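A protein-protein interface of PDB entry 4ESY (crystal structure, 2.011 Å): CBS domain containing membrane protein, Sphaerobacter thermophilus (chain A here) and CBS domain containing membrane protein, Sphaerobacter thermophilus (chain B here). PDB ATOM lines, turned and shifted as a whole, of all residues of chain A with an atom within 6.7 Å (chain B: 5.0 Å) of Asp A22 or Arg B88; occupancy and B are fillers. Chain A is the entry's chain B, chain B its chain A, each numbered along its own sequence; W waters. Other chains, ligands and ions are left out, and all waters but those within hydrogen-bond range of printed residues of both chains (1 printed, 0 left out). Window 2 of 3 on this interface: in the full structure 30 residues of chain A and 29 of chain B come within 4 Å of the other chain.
CG2 of Val A18 touches CB of Ala B89 (3.9 Å). Asp A22 touches Trp B78 (O to CH2, 3.2 Å). Asp A22 touches Ile B85. Ile A23 touches Trp B78 (CA to CH2, 3.9 Å). Trp B78 touches Thr A25 (CZ2 to CG2, 3.9 Å).
Water W1 bridges the side-chain carboxylate (OD2) of Asp A22 (2.7 Å) and the backbone carbonyl oxygen (O) of Ile B85 (2.9 Å).
The guanidinium group of Arg B88 lies within salt-bridge range of the side-chain carboxylate of Asp A22 (3.6 Å).
Hydrophobic or aromatic side chains of chain B that line the printed part of chain A: Trp B78, Ile B85 and Ala B89. Hydrophobic or aromatic side chains of chain A within 4 Å of the printed part of chain B: Val A18 and Ile A23. Among the printed residues, 6 pairs touch across the chains. Among the printed residues, Asp or Glu carboxylates within 4 Å of a Lys or Arg side-chain nitrogen of the other chain: Asp A22 with Arg B88.
Of chain B, only Trp B78 (3.2 Å), Ile B85 (3.9 Å) and Arg B88 (3.6 Å) come within 4 Å of Asp A22. Of the printed residues of chain B, Val A18 touches Ala B89. Printed residues of chain A within 4 Å of Trp B78: Asp A22 (3.2 Å), Ile A23 (3.9 Å) and Thr A25 (3.9 Å). The nearest printed residue of chain B that does not touch Asp A22 is Ala B89 (6.7 Å). The nearest printed residue of chain A that does not touch Arg B88 is Val A18 (6.9 Å). The nearest printed residue of chain B that does not touch Ile A23 is Ile B85 (5.7 Å).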
ATOM      1  N   VAL A  18     -16.818 -15.227   0.883  1.00  0.00           N
ATOM      2  CA  VAL A  18     -16.821 -14.314  -0.270  1.00  0.00           C
ATOM      3  C   VAL A  18     -15.595 -13.379  -0.272  1.00  0.00           C
ATOM      4  O   VAL A  18     -15.286 -12.753   0.732  1.00  0.00           O
ATOM      5  CB  VAL A  18     -18.101 -13.468  -0.227  1.00  0.00           C
ATOM      6  CG1 VAL A  18     -18.070 -12.326  -1.271  1.00  0.00           C
ATOM      7  CG2 VAL A  18     -19.351 -14.379  -0.368  1.00  0.00           C
ATOM      8  N   PRO A  19     -14.872 -13.283  -1.396  1.00  0.00           N
ATOM      9  CA  PRO A  19     -13.715 -12.373  -1.287  1.00  0.00           C
ATOM     10  C   PRO A  19     -14.159 -10.918  -1.326  1.00  0.00           C
ATOM     11  O   PRO A  19     -15.140 -10.585  -1.997  1.00  0.00           O
ATOM     12  CB  PRO A  19     -12.842 -12.716  -2.507  1.00  0.00           C
ATOM     13  CG  PRO A  19     -13.775 -13.422  -3.467  1.00  0.00           C
ATOM     14  CD  PRO A  19     -14.863 -14.080  -2.631  1.00  0.00           C
ATOM     15  N   ILE A  20     -13.449 -10.082  -0.576  1.00  0.00           N
ATOM     16  CA  ILE A  20     -13.695  -8.643  -0.556  1.00  0.00           C
ATOM     17  C   ILE A  20     -13.919  -8.028  -1.923  1.00  0.00           C
ATOM     18  O   ILE A  20     -14.855  -7.257  -2.107  1.00  0.00           O
ATOM     19  CB  ILE A  20     -12.550  -7.865   0.152  1.00  0.00           C
ATOM     20  CG1 ILE A  20     -12.633  -8.109   1.643  1.00  0.00           C
ATOM     21  CG2 ILE A  20     -12.710  -6.366  -0.059  1.00  0.00           C
ATOM     22  CD1 ILE A  20     -14.018  -7.805   2.136  1.00  0.00           C
ATOM     23  N   ARG A  21     -13.076  -8.369  -2.887  1.00  0.00           N
ATOM     24  CA  ARG A  21     -13.185  -7.725  -4.198  1.00  0.00           C
ATOM     25  C   ARG A  21     -14.590  -7.898  -4.814  1.00  0.00           C
ATOM     26  O   ARG A  21     -15.009  -7.086  -5.631  1.00  0.00           O
ATOM     27  CB  ARG A  21     -12.066  -8.172  -5.158  1.00  0.00           C
ATOM     28  CG  ARG A  21     -12.499  -9.178  -6.217  1.00  0.00           C
ATOM     29  CD  ARG A  21     -11.312  -9.888  -6.856  1.00  0.00           C
ATOM     30  NE  ARG A  21     -11.106 -11.192  -6.233  1.00  0.00           N
ATOM     31  CZ  ARG A  21      -9.943 -11.618  -5.754  1.00  0.00           C
ATOM     32  NH1 ARG A  21      -8.861 -10.846  -5.843  1.00  0.00           N
ATOM     33  NH2 ARG A  21      -9.866 -12.820  -5.189  1.00  0.00           N
ATOM     34  N   ASP A  22     -15.329  -8.923  -4.374  1.00  0.00           N
ATOM     35  CA  ASP A  22     -16.698  -9.162  -4.855  1.00  0.00           C
ATOM     36  C   ASP A  22     -17.716  -8.149  -4.305  1.00  0.00           C
ATOM     37  O   ASP A  22     -18.769  -7.977  -4.877  1.00  0.00           O
ATOM     38  CB  ASP A  22     -17.168 -10.582  -4.522  1.00  0.00           C
ATOM     39  CG  ASP A  22     -16.617 -11.626  -5.475  1.00  0.00           C
ATOM     40  OD1 ASP A  22     -15.939 -11.268  -6.467  1.00  0.00           O
ATOM     41  OD2 ASP A  22     -16.886 -12.820  -5.245  1.00  0.00           O
ATOM     42  N   ILE A  23     -17.406  -7.489  -3.194  1.00  0.00           N
ATOM     43  CA  ILE A  23     -18.339  -6.527  -2.640  1.00  0.00           C
ATOM     44  C   ILE A  23     -17.981  -5.087  -2.982  1.00  0.00           C
ATOM     45  O   ILE A  23     -18.764  -4.174  -2.690  1.00  0.00           O
ATOM     46  CB  ILE A  23     -18.563  -6.683  -1.117  1.00  0.00           C
ATOM     47  CG1 ILE A  23     -17.382  -6.167  -0.298  1.00  0.00           C
ATOM     48  CG2 ILE A  23     -18.843  -8.146  -0.769  1.00  0.00           C
ATOM     49  CD1 ILE A  23     -17.656  -6.191   1.240  1.00  0.00           C
ATOM     50  N   LEU A  24     -16.832  -4.885  -3.627  1.00  0.00           N
ATOM     51  CA  LEU A  24     -16.455  -3.555  -4.090  1.00  0.00           C
ATOM     52  C   LEU A  24     -17.103  -3.296  -5.432  1.00  0.00           C
ATOM     53  O   LEU A  24     -16.476  -3.471  -6.468  1.00  0.00           O
ATOM     54  CB  LEU A  24     -14.935  -3.440  -4.226  1.00  0.00           C
ATOM     55  CG  LEU A  24     -14.224  -3.573  -2.886  1.00  0.00           C
ATOM     56  CD1 LEU A  24     -12.705  -3.509  -3.069  1.00  0.00           C
ATOM     57  CD2 LEU A  24     -14.713  -2.483  -1.916  1.00  0.00           C
ATOM     58  N   THR A  25     -18.361  -2.888  -5.420  1.00  0.00           N
ATOM     59  CA  THR A  25     -19.156  -2.828  -6.651  1.00  0.00           C
ATOM     60  C   THR A  25     -19.320  -1.392  -7.132  1.00  0.00           C
ATOM     61  O   THR A  25     -19.994  -1.116  -8.131  1.00  0.00           O
ATOM     62  CB  THR A  25     -20.549  -3.426  -6.433  1.00  0.00           C
ATOM     63  OG1 THR A  25     -21.208  -2.684  -5.404  1.00  0.00           O
ATOM     64  CG2 THR A  25     -20.453  -4.920  -6.024  1.00  0.00           C
ATOM     65  N   PRO A 120      -7.859  -7.085  -1.532  1.00  0.00           N
ATOM     66  CA  PRO A 120      -9.101  -7.538  -2.184  1.00  0.00           C
ATOM     67  C   PRO A 120      -9.318  -9.069  -2.194  1.00  0.00           C
ATOM     68  O   PRO A 120     -10.443  -9.568  -2.377  1.00  0.00           O
ATOM     69  CB  PRO A 120      -8.958  -6.983  -3.611  1.00  0.00           C
ATOM     70  CG  PRO A 120      -7.496  -6.788  -3.804  1.00  0.00           C
ATOM     71  CD  PRO A 120      -6.995  -6.336  -2.467  1.00  0.00           C
ATOM     72  N   TRP B  78     -28.190  -7.993   0.795  1.00  0.00           N
ATOM     73  CA  TRP B  78     -27.387  -7.958  -0.440  1.00  0.00           C
ATOM     74  C   TRP B  78     -27.956  -8.843  -1.558  1.00  0.00           C
ATOM     75  O   TRP B  78     -27.724  -8.597  -2.752  1.00  0.00           O
ATOM     76  CB  TRP B  78     -25.915  -8.325  -0.154  1.00  0.00           C
ATOM     77  CG  TRP B  78     -24.977  -7.558  -1.059  1.00  0.00           C
ATOM     78  CD1 TRP B  78     -25.065  -6.225  -1.378  1.00  0.00           C
ATOM     79  CD2 TRP B  78     -23.885  -8.087  -1.829  1.00  0.00           C
ATOM     80  NE1 TRP B  78     -24.068  -5.889  -2.271  1.00  0.00           N
ATOM     81  CE2 TRP B  78     -23.333  -7.010  -2.565  1.00  0.00           C
ATOM     82  CE3 TRP B  78     -23.313  -9.360  -1.957  1.00  0.00           C
ATOM     83  CZ2 TRP B  78     -22.228  -7.166  -3.421  1.00  0.00           C
ATOM     84  CZ3 TRP B  78     -22.221  -9.520  -2.795  1.00  0.00           C
ATOM     85  CH2 TRP B  78     -21.676  -8.423  -3.511  1.00  0.00           C
ATOM     86  N   GLU B  84     -26.551 -12.418  -8.397  1.00  0.00           N
ATOM     87  CA  GLU B  84     -25.628 -13.095  -9.294  1.00  0.00           C
ATOM     88  C   GLU B  84     -24.247 -13.302  -8.658  1.00  0.00           C
ATOM     89  O   GLU B  84     -23.648 -14.370  -8.791  1.00  0.00           O
ATOM     90  CB  GLU B  84     -25.543 -12.371 -10.638  1.00  0.00           C
ATOM     91  CG  GLU B  84     -24.933 -10.982 -10.611  1.00  0.00           C
ATOM     92  CD  GLU B  84     -25.592 -10.018  -9.637  1.00  0.00           C
ATOM     93  OE1 GLU B  84     -26.862  -9.905  -9.605  1.00  0.00           O
ATOM     94  OE2 GLU B  84     -24.805  -9.379  -8.896  1.00  0.00           O
ATOM     95  N   ILE B  85     -23.769 -12.296  -7.929  1.00  0.00           N
ATOM     96  CA  ILE B  85     -22.478 -12.393  -7.270  1.00  0.00           C
ATOM     97  C   ILE B  85     -22.567 -13.405  -6.137  1.00  0.00           C
ATOM     98  O   ILE B  85     -21.706 -14.241  -5.991  1.00  0.00           O
ATOM     99  CB  ILE B  85     -21.947 -11.010  -6.801  1.00  0.00           C
ATOM    100  CG1 ILE B  85     -21.465 -10.214  -8.020  1.00  0.00           C
ATOM    101  CG2 ILE B  85     -20.734 -11.191  -5.915  1.00  0.00           C
ATOM    102  CD1 ILE B  85     -21.702  -8.725  -7.912  1.00  0.00           C
ATOM    103  N   LEU B  86     -23.656 -13.354  -5.389  1.00  0.00           N
ATOM    104  CA  LEU B  86     -23.861 -14.273  -4.282  1.00  0.00           C
ATOM    105  C   LEU B  86     -24.126 -15.706  -4.730  1.00  0.00           C
ATOM    106  O   LEU B  86     -23.742 -16.662  -4.045  1.00  0.00           O
ATOM    107  CB  LEU B  86     -24.956 -13.765  -3.345  1.00  0.00           C
ATOM    108  CG  LEU B  86     -24.490 -12.599  -2.457  1.00  0.00           C
ATOM    109  CD1 LEU B  86     -25.599 -12.151  -1.445  1.00  0.00           C
ATOM    110  CD2 LEU B  86     -23.206 -12.919  -1.705  1.00  0.00           C
ATOM    111  N   SER B  87     -24.722 -15.864  -5.906  1.00  0.00           N
ATOM    112  CA  SER B  87     -24.891 -17.201  -6.476  1.00  0.00           C
ATOM    113  C   SER B  87     -23.591 -17.906  -6.804  1.00  0.00           C
ATOM    114  O   SER B  87     -23.578 -19.104  -7.065  1.00  0.00           O
ATOM    115  CB  SER B  87     -25.805 -17.154  -7.687  1.00  0.00           C
ATOM    116  OG  SER B  87     -27.071 -16.659  -7.254  1.00  0.00           O
ATOM    117  N   ARG B  88     -22.489 -17.170  -6.789  1.00  0.00           N
ATOM    118  CA  ARG B  88     -21.195 -17.798  -6.977  1.00  0.00           C
ATOM    119  C   ARG B  88     -20.765 -18.500  -5.704  1.00  0.00           C
ATOM    120  O   ARG B  88     -19.949 -19.406  -5.736  1.00  0.00           O
ATOM    121  CB  ARG B  88     -20.147 -16.778  -7.410  1.00  0.00           C
ATOM    122  CG  ARG B  88     -19.943 -16.772  -8.886  1.00  0.00           C
ATOM    123  CD  ARG B  88     -20.161 -15.412  -9.482  1.00  0.00           C
ATOM    124  NE  ARG B  88     -19.110 -14.475  -9.100  1.00  0.00           N
ATOM    125  CZ  ARG B  88     -18.964 -13.264  -9.636  1.00  0.00           C
ATOM    126  NH1 ARG B  88     -17.984 -12.484  -9.202  1.00  0.00           N
ATOM    127  NH2 ARG B  88     -19.770 -12.846 -10.617  1.00  0.00           N
ATOM    128  N   ALA B  89     -21.334 -18.060  -4.586  1.00  0.00           N
ATOM    129  CA  ALA B  89     -20.964 -18.569  -3.286  1.00  0.00           C
ATOM    130  C   ALA B  89     -21.978 -19.589  -2.763  1.00  0.00           C
ATOM    131  O   ALA B  89     -21.610 -20.565  -2.131  1.00  0.00           O
ATOM    132  CB  ALA B  89     -20.816 -17.418  -2.315  1.00  0.00           C
ATOM    133  N   ILE B  90     -23.252 -19.347  -3.051  1.00  0.00           N
ATOM    134  CA  ILE B  90     -24.375 -20.111  -2.523  1.00  0.00           C
ATOM    135  C   ILE B  90     -25.089 -20.808  -3.677  1.00  0.00           C
ATOM    136  O   ILE B  90     -25.417 -20.159  -4.670  1.00  0.00           O
ATOM    137  CB  ILE B  90     -25.378 -19.153  -1.888  1.00  0.00           C
ATOM    138  CG1 ILE B  90     -24.676 -18.189  -0.934  1.00  0.00           C
ATOM    139  CG2 ILE B  90     -26.461 -19.891  -1.150  1.00  0.00           C
ATOM    140  CD1 ILE B  90     -25.588 -17.050  -0.404  1.00  0.00           C
HETATM  141  O   HOH W   1     -19.160 -14.216  -4.618  1.00  0.00           O
